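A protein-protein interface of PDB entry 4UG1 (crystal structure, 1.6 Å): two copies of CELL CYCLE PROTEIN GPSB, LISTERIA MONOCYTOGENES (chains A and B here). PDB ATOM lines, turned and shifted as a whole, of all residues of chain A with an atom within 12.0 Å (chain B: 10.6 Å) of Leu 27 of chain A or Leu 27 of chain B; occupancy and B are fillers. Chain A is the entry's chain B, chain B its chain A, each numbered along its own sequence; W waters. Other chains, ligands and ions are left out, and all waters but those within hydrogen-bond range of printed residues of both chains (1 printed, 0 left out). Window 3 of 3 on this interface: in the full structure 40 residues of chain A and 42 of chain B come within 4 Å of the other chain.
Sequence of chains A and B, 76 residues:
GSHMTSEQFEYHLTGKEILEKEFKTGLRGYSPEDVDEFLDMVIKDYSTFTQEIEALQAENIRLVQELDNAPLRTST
The backbone NH (N) of Arg 28 of chain A lies close to the backbone carbonyl oxygen (O) of Gly 26 of chain B (3.3 Å).
The backbone carbonyl oxygen (O) of Tyr 30 of chain A sits at hydrogen-bond distance from the backbone NH (N) of Tyr 30 of chain B (2.9 Å).
The backbone NH of Gly 26 of chain B is in hydrogen-bond range of the backbone carbonyl oxygen of Gly 29 of chain A, at 3.1 Å.
O of Lys 24 of chain A is in hydrogen-bond range of N of Ser 31 of chain B (2.7 Å).
The backbone carbonyl oxygen (O) of Lys 24 of chain B sits at hydrogen-bond distance from the backbone NH (N) of Ser 31 of chain A (2.8 Å).
N of Gly 26 of chain A sits at hydrogen-bond distance from O of Gly 29 of chain B.
N of Lys 24 of chain B is in hydrogen-bond range of OD2 of Asp 34 of chain A (3.4 Å).
The backbone carbonyl oxygen (O) of Leu 27 of chain B lies within hydrogen-bond range of the backbone NH (N) of Arg 28 of chain A (2.9 Å).
The guanidinium group (NH1) of Arg 28 of chain B is in hydrogen-bond range of the side-chain hydroxyl (OG1) of Thr 25 of chain A (3.2 Å).
The backbone NH (N) of Asp 34 of chain A sits at hydrogen-bond distance from the side-chain hydroxyl (OG) of Ser 31 of chain A (3.1 Å).
The side-chain hydroxyl (OG) of Ser 31 of chain A sits at hydrogen-bond distance from the side-chain carboxylate (OE1) of Glu 33 of chain A.
Among the printed residues, pairs that only touch across the chains: Phe 23 of chain A with Tyr 30 of chain B (3.7 Å), Lys 24 of chain A with Tyr 30 of chain B (3.5 Å), Thr 25 of chain A with Gly 29 of chain B (3.1 Å), Gly 26 of chain A with Leu 27 of chain B (3.97 Å), Gly 26 of chain A with Arg 28 of chain B (3.4 Å), Leu 27 of chain A with Leu 27 of chain B (3.3 Å), Arg 28 of chain A with Thr 25 of chain B (3.8 Å), Gly 29 of chain A with Thr 25 of chain B (3.2 Å), Gly 29 of chain A with Gly 29 of chain B (3.6 Å), Gly 29 of chain A with Tyr 30 of chain B (3.2 Å), Gly 29 of chain A with Pro 32 of chain B (3.9 Å), Tyr 30 of chain A with Lys 24 of chain B (3.4 Å), Tyr 30 of chain A with Gly 29 of chain B (3.3 Å), Tyr 30 of chain A with Pro 32 of chain B (3.6 Å) and Pro 32 of chain A with Tyr 30 of chain B (3.7 Å).
Printed residues of chain B within 4 Å of Lys 24 of chain A: Tyr 30 and Ser 31.
Gly 26 of chain A touches just these residues of chain B: Leu 27 (3.97 Å), Arg 28 (3.4 Å) and Gly 29 (2.9 Å).
Of chain B, only Leu 27 (3.3 Å) comes within 4 Å of Leu 27 of chain A.
Printed residues of chain B within 4 Å of Arg 28 of chain A: Thr 25 (3.8 Å), Gly 26 (3.1 Å) and Leu 27 (2.9 Å).
Gly 29 of chain A touches just these residues of chain B: Thr 25 (3.2 Å), Gly 26 (3.1 Å), Gly 29 (3.6 Å), Tyr 30 (3.2 Å) and Pro 32 (3.9 Å).
Of the printed residues of chain B, Ser 31 of chain A touches Lys 24.
Of the printed residues of chain B, Asp 34 of chain A touches Lys 24 (3.4 Å).
Thr 25 of chain B touches just these residues of chain A: Arg 28 and Gly 29.
Of chain A, only Arg 28 and Gly 29 come within 4 Å of Gly 26 of chain B.
Leu 27 of chain B touches just these residues of chain A: Gly 26 (3.97 Å), Leu 27 (3.3 Å) and Arg 28 (2.9 Å).
Arg 28 of chain B touches just these residues of chain A: Thr 25 and Gly 26.
Gly 29 of chain B touches four residues of chain A.
The nearest residue of chain B that does not touch Leu 27 of chain A is Arg 28 of chain B (4.2 Å).
The nearest residue of chain A that does not touch Leu 27 of chain B is Gly 29 of chain A (4.8 Å).
The nearest printed residue of chain A that does not touch Tyr 30 of chain B is Thr 25 of chain A (4.4 Å).
Printed residues of chain B that touch a printed residue of chain A: Lys 24, Thr 25, Gly 26, Leu 27, Arg 28, Gly 29, Tyr 30, Ser 31 and Pro 32.
Hydrophobic or aromatic side chains of chain B that line the printed part of chain A: Tyr 30 and Pro 32.
Hydrophobic or aromatic side chains of chain A within 4 Å of the printed part of chain B: Phe 23, Leu 27, Tyr 30 and Pro 32.
Lys 24 of chain A touches Tyr 30 of chain B, and with the chains exchanged Tyr 30 of chain A touches Lys 24 of chain B.
Lys 24 of chain A touches Ser 31 of chain B, and with the chains exchanged Ser 31 of chain A touches Lys 24 of chain B.
Leu 27 of chain A touches its own counterpart, Leu 27 of chain B.
Tyr 30 of chain B touches its own counterpart, Tyr 30 of chain A.
Of the 24 pairs that touch across the chains among the printed residues, 19 have their exchanged pair printed and touching as well.
Water W1 bridges OH of Tyr 30 of chain B and N of Phe 23 of chain A.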
ATOM      1  N   PHE A  23     -16.442  24.228  20.415  1.00  0.00           N
ATOM      2  CA  PHE A  23     -15.639  25.025  19.496  1.00  0.00           C
ATOM      3  C   PHE A  23     -16.491  25.819  18.519  1.00  0.00           C
ATOM      4  O   PHE A  23     -17.547  25.364  18.076  1.00  0.00           O
ATOM      5  CB  PHE A  23     -14.669  24.139  18.712  1.00  0.00           C
ATOM      6  CG  PHE A  23     -13.655  23.455  19.572  1.00  0.00           C
ATOM      7  CD1 PHE A  23     -12.539  24.143  20.028  1.00  0.00           C
ATOM      8  CD2 PHE A  23     -13.833  22.143  19.951  1.00  0.00           C
ATOM      9  CE1 PHE A  23     -11.600  23.513  20.834  1.00  0.00           C
ATOM     10  CE2 PHE A  23     -12.901  21.506  20.770  1.00  0.00           C
ATOM     11  CZ  PHE A  23     -11.784  22.198  21.207  1.00  0.00           C
ATOM     12  N   LYS A  24     -16.026  27.018  18.198  1.00  0.00           N
ATOM     13  CA  LYS A  24     -16.598  27.784  17.099  1.00  0.00           C
ATOM     14  C   LYS A  24     -16.433  26.998  15.801  1.00  0.00           C
ATOM     15  O   LYS A  24     -15.437  26.292  15.617  1.00  0.00           O
ATOM     16  CB  LYS A  24     -15.928  29.153  16.982  1.00  0.00           C
ATOM     17  N   THR A  25     -17.417  27.092  14.915  1.00  0.00           N
ATOM     18  CA  THR A  25     -17.293  26.455  13.612  1.00  0.00           C
ATOM     19  C   THR A  25     -16.980  27.476  12.536  1.00  0.00           C
ATOM     20  O   THR A  25     -17.156  28.684  12.723  1.00  0.00           O
ATOM     21  CB  THR A  25     -18.565  25.705  13.194  1.00  0.00           C
ATOM     22  OG1 THR A  25     -19.602  26.645  12.891  1.00  0.00           O
ATOM     23  CG2 THR A  25     -19.020  24.758  14.287  1.00  0.00           C
ATOM     24  N   GLY A  26     -16.516  26.978  11.400  1.00  0.00           N
ATOM     25  CA  GLY A  26     -16.298  27.817  10.246  1.00  0.00           C
ATOM     26  C   GLY A  26     -16.126  26.983   9.000  1.00  0.00           C
ATOM     27  O   GLY A  26     -16.124  25.754   9.057  1.00  0.00           O
ATOM     28  N   LEU A  27     -15.981  27.652   7.866  1.00  0.00           N
ATOM     29  CA  LEU A  27     -15.651  26.967   6.625  1.00  0.00           C
ATOM     30  C   LEU A  27     -14.312  26.260   6.757  1.00  0.00           C
ATOM     31  O   LEU A  27     -13.358  26.834   7.273  1.00  0.00           O
ATOM     32  CB  LEU A  27     -15.600  27.958   5.462  1.00  0.00           C
ATOM     33  CG  LEU A  27     -16.918  28.523   4.946  1.00  0.00           C
ATOM     34  CD1 LEU A  27     -16.639  29.465   3.807  1.00  0.00           C
ATOM     35  CD2 LEU A  27     -17.829  27.400   4.504  1.00  0.00           C
ATOM     36  N   ARG A  28     -14.253  25.019   6.285  1.00  0.00           N
ATOM     37  CA  ARG A  28     -13.007  24.259   6.194  1.00  0.00           C
ATOM     38  C   ARG A  28     -12.370  24.020   7.544  1.00  0.00           C
ATOM     39  O   ARG A  28     -11.145  23.979   7.677  1.00  0.00           O
ATOM     40  CB  ARG A  28     -12.009  24.956   5.296  1.00  0.00           C
ATOM     41  CG  ARG A  28     -12.430  24.971   3.878  1.00  0.00           C
ATOM     42  CD  ARG A  28     -11.261  25.284   3.013  1.00  0.00           C
ATOM     43  NE  ARG A  28     -11.708  25.753   1.718  1.00  0.00           N
ATOM     44  CZ  ARG A  28     -10.913  25.895   0.671  1.00  0.00           C
ATOM     45  NH1 ARG A  28      -9.623  25.602   0.772  1.00  0.00           N
ATOM     46  NH2 ARG A  28     -11.410  26.330  -0.471  1.00  0.00           N
ATOM     47  N   GLY A  29     -13.203  23.857   8.549  1.00  0.00           N
ATOM     48  CA  GLY A  29     -12.666  23.529   9.847  1.00  0.00           C
ATOM     49  C   GLY A  29     -12.296  22.061   9.979  1.00  0.00           C
ATOM     50  O   GLY A  29     -12.548  21.249   9.085  1.00  0.00           O
ATOM     51  N   TYR A  30     -11.697  21.732  11.117  1.00  0.00           N
ATOM     52  CA  TYR A  30     -11.400  20.347  11.463  1.00  0.00           C
ATOM     53  C   TYR A  30     -12.673  19.527  11.602  1.00  0.00           C
ATOM     54  O   TYR A  30     -13.651  19.995  12.174  1.00  0.00           O
ATOM     55  CB  TYR A  30     -10.639  20.275  12.781  1.00  0.00           C
ATOM     56  CG  TYR A  30      -9.266  20.894  12.799  1.00  0.00           C
ATOM     57  CD1 TYR A  30      -8.521  21.052  11.636  1.00  0.00           C
ATOM     58  CD2 TYR A  30      -8.698  21.294  14.005  1.00  0.00           C
ATOM     59  CE1 TYR A  30      -7.246  21.609  11.678  1.00  0.00           C
ATOM     60  CE2 TYR A  30      -7.445  21.846  14.060  1.00  0.00           C
ATOM     61  CZ  TYR A  30      -6.714  22.007  12.898  1.00  0.00           C
ATOM     62  OH  TYR A  30      -5.451  22.558  12.962  1.00  0.00           O
ATOM     63  N   SER A  31     -12.640  18.290  11.121  1.00  0.00           N
ATOM     64  CA  SER A  31     -13.766  17.372  11.267  1.00  0.00           C
ATOM     65  C   SER A  31     -14.211  17.256  12.720  1.00  0.00           C
ATOM     66  O   SER A  31     -13.436  16.822  13.561  1.00  0.00           O
ATOM     67  CB  SER A  31     -13.389  15.992  10.749  1.00  0.00           C
ATOM     68  OG  SER A  31     -14.250  15.004  11.287  1.00  0.00           O
ATOM     69  N   PRO A  32     -15.462  17.635  13.018  1.00  0.00           N
ATOM     70  CA  PRO A  32     -15.922  17.527  14.411  1.00  0.00           C
ATOM     71  C   PRO A  32     -15.828  16.113  14.967  1.00  0.00           C
ATOM     72  O   PRO A  32     -15.447  15.934  16.124  1.00  0.00           O
ATOM     73  CB  PRO A  32     -17.379  17.982  14.331  1.00  0.00           C
ATOM     74  CG  PRO A  32     -17.391  18.930  13.162  1.00  0.00           C
ATOM     75  CD  PRO A  32     -16.471  18.278  12.156  1.00  0.00           C
ATOM     76  N   GLU A  33     -16.156  15.128  14.140  1.00  0.00           N
ATOM     77  CA  GLU A  33     -16.103  13.727  14.539  1.00  0.00           C
ATOM     78  C   GLU A  33     -14.681  13.311  14.901  1.00  0.00           C
ATOM     79  O   GLU A  33     -14.465  12.635  15.915  1.00  0.00           O
ATOM     80  CB  GLU A  33     -16.654  12.839  13.414  1.00  0.00           C
ATOM     81  CG  GLU A  33     -18.119  13.106  13.052  1.00  0.00           C
ATOM     82  CD  GLU A  33     -18.342  14.401  12.264  1.00  0.00           C
ATOM     83  OE1 GLU A  33     -17.483  14.775  11.434  1.00  0.00           O
ATOM     84  OE2 GLU A  33     -19.388  15.049  12.482  1.00  0.00           O
ATOM     85  N   ASP A  34     -13.722  13.722  14.074  1.00  0.00           N
ATOM     86  CA  ASP A  34     -12.299  13.430  14.279  1.00  0.00           C
ATOM     87  C   ASP A  34     -11.764  14.078  15.563  1.00  0.00           C
ATOM     88  O   ASP A  34     -11.081  13.425  16.355  1.00  0.00           O
ATOM     89  CB  ASP A  34     -11.493  13.915  13.067  1.00  0.00           C
ATOM     90  CG  ASP A  34     -10.140  13.232  12.935  1.00  0.00           C
ATOM     91  OD1 ASP A  34      -9.781  12.413  13.809  1.00  0.00           O
ATOM     92  OD2 ASP A  34      -9.430  13.527  11.946  1.00  0.00           O
ATOM     93  N   LYS B  24      -8.400  15.862   9.659  1.00  0.00           N
ATOM     94  CA  LYS B  24      -9.041  16.091   8.373  1.00  0.00           C
ATOM     95  C   LYS B  24      -9.901  17.350   8.448  1.00  0.00           C
ATOM     96  O   LYS B  24     -10.351  17.740   9.528  1.00  0.00           O
ATOM     97  CB  LYS B  24      -9.895  14.890   7.963  1.00  0.00           C
ATOM     98  N   THR B  25     -10.113  17.989   7.302  1.00  0.00           N
ATOM     99  CA  THR B  25     -10.971  19.169   7.234  1.00  0.00           C
ATOM    100  C   THR B  25     -12.165  18.907   6.333  1.00  0.00           C
ATOM    101  O   THR B  25     -12.083  18.116   5.392  1.00  0.00           O
ATOM    102  CB  THR B  25     -10.221  20.413   6.715  1.00  0.00           C
ATOM    103  OG1 THR B  25      -9.828  20.211   5.353  1.00  0.00           O
ATOM    104  CG2 THR B  25      -8.993  20.699   7.567  1.00  0.00           C
ATOM    105  N   GLY B  26     -13.273  19.579   6.624  1.00  0.00           N
ATOM    106  CA  GLY B  26     -14.497  19.391   5.871  1.00  0.00           C
ATOM    107  C   GLY B  26     -15.200  20.713   5.677  1.00  0.00           C
ATOM    108  O   GLY B  26     -14.774  21.713   6.246  1.00  0.00           O
ATOM    109  N   LEU B  27     -16.282  20.700   4.902  1.00  0.00           N
ATOM    110  CA  LEU B  27     -16.967  21.919   4.473  1.00  0.00           C
ATOM    111  C   LEU B  27     -17.217  22.879   5.626  1.00  0.00           C
ATOM    112  O   LEU B  27     -16.882  24.065   5.547  1.00  0.00           O
ATOM    113  CB  LEU B  27     -18.288  21.573   3.787  1.00  0.00           C
ATOM    114  CG  LEU B  27     -19.111  22.759   3.287  1.00  0.00           C
ATOM    115  CD1 LEU B  27     -18.250  23.679   2.436  1.00  0.00           C
ATOM    116  CD2 LEU B  27     -20.319  22.280   2.503  1.00  0.00           C
ATOM    117  N   ARG B  28     -17.821  22.358   6.688  1.00  0.00           N
ATOM    118  CA  ARG B  28     -17.945  23.060   7.951  1.00  0.00           C
ATOM    119  C   ARG B  28     -17.173  22.216   8.954  1.00  0.00           C
ATOM    120  O   ARG B  28     -17.153  20.990   8.849  1.00  0.00           O
ATOM    121  CB  ARG B  28     -19.404  23.212   8.394  1.00  0.00           C
ATOM    122  CG  ARG B  28     -20.138  24.420   7.830  1.00  0.00           C
ATOM    123  CD  ARG B  28     -20.214  25.555   8.846  1.00  0.00           C
ATOM    124  NE  ARG B  28     -20.323  26.844   8.176  1.00  0.00           N
ATOM    125  CZ  ARG B  28     -20.043  28.011   8.742  1.00  0.00           C
ATOM    126  NH1 ARG B  28     -19.640  28.064  10.004  1.00  0.00           N
ATOM    127  NH2 ARG B  28     -20.159  29.126   8.040  1.00  0.00           N
ATOM    128  N   GLY B  29     -16.527  22.861   9.906  1.00  0.00           N
ATOM    129  CA  GLY B  29     -15.829  22.125  10.943  1.00  0.00           C
ATOM    130  C   GLY B  29     -15.450  23.045  12.077  1.00  0.00           C
ATOM    131  O   GLY B  29     -15.744  24.231  12.041  1.00  0.00           O
ATOM    132  N   TYR B  30     -14.799  22.494  13.095  1.00  0.00           N
ATOM    133  CA  TYR B  30     -14.312  23.306  14.197  1.00  0.00           C
ATOM    134  C   TYR B  30     -13.208  24.260  13.744  1.00  0.00           C
ATOM    135  O   TYR B  30     -12.333  23.867  12.979  1.00  0.00           O
ATOM    136  CB  TYR B  30     -13.763  22.420  15.315  1.00  0.00           C
ATOM    137  CG  TYR B  30     -14.750  21.521  16.022  1.00  0.00           C
ATOM    138  CD1 TYR B  30     -16.104  21.816  16.078  1.00  0.00           C
ATOM    139  CD2 TYR B  30     -14.299  20.384  16.684  1.00  0.00           C
ATOM    140  CE1 TYR B  30     -16.996  20.973  16.751  1.00  0.00           C
ATOM    141  CE2 TYR B  30     -15.170  19.552  17.360  1.00  0.00           C
ATOM    142  CZ  TYR B  30     -16.512  19.846  17.398  1.00  0.00           C
ATOM    143  OH  TYR B  30     -17.358  18.998  18.080  1.00  0.00           O
ATOM    144  N   SER B  31     -13.240  25.499  14.236  1.00  0.00           N
ATOM    145  CA  SER B  31     -12.193  26.475  13.941  1.00  0.00           C
ATOM    146  C   SER B  31     -10.806  25.902  14.213  1.00  0.00           C
ATOM    147  O   SER B  31     -10.506  25.536  15.349  1.00  0.00           O
ATOM    148  CB  SER B  31     -12.404  27.739  14.777  1.00  0.00           C
ATOM    149  OG  SER B  31     -11.188  28.445  14.970  1.00  0.00           O
ATOM    150  N   PRO B  32      -9.963  25.792  13.172  1.00  0.00           N
ATOM    151  CA  PRO B  32      -8.630  25.223  13.402  1.00  0.00           C
ATOM    152  C   PRO B  32      -7.821  26.020  14.421  1.00  0.00           C
ATOM    153  O   PRO B  32      -7.157  25.418  15.273  1.00  0.00           O
ATOM    154  CB  PRO B  32      -7.990  25.263  12.005  1.00  0.00           C
ATOM    155  CG  PRO B  32      -9.145  25.133  11.086  1.00  0.00           C
ATOM    156  CD  PRO B  32     -10.242  25.953  11.732  1.00  0.00           C
ATOM    157  N   GLU B  33      -7.901  27.345  14.371  1.00  0.00           N
ATOM    158  CA  GLU B  33      -7.161  28.174  15.314  1.00  0.00           C
ATOM    159  C   GLU B  33      -7.595  27.904  16.753  1.00  0.00           C
ATOM    160  O   GLU B  33      -6.766  27.805  17.658  1.00  0.00           O
ATOM    161  CB  GLU B  33      -7.335  29.658  14.976  1.00  0.00           C
ATOM    162  CG  GLU B  33      -6.464  30.576  15.798  1.00  0.00           C
ATOM    163  CD  GLU B  33      -6.740  32.041  15.522  1.00  0.00           C
ATOM    164  OE1 GLU B  33      -7.595  32.336  14.657  1.00  0.00           O
ATOM    165  OE2 GLU B  33      -6.105  32.900  16.172  1.00  0.00           O
HETATM  166  O   HOH W   1     -17.680  21.361  20.022  1.00  0.00           O
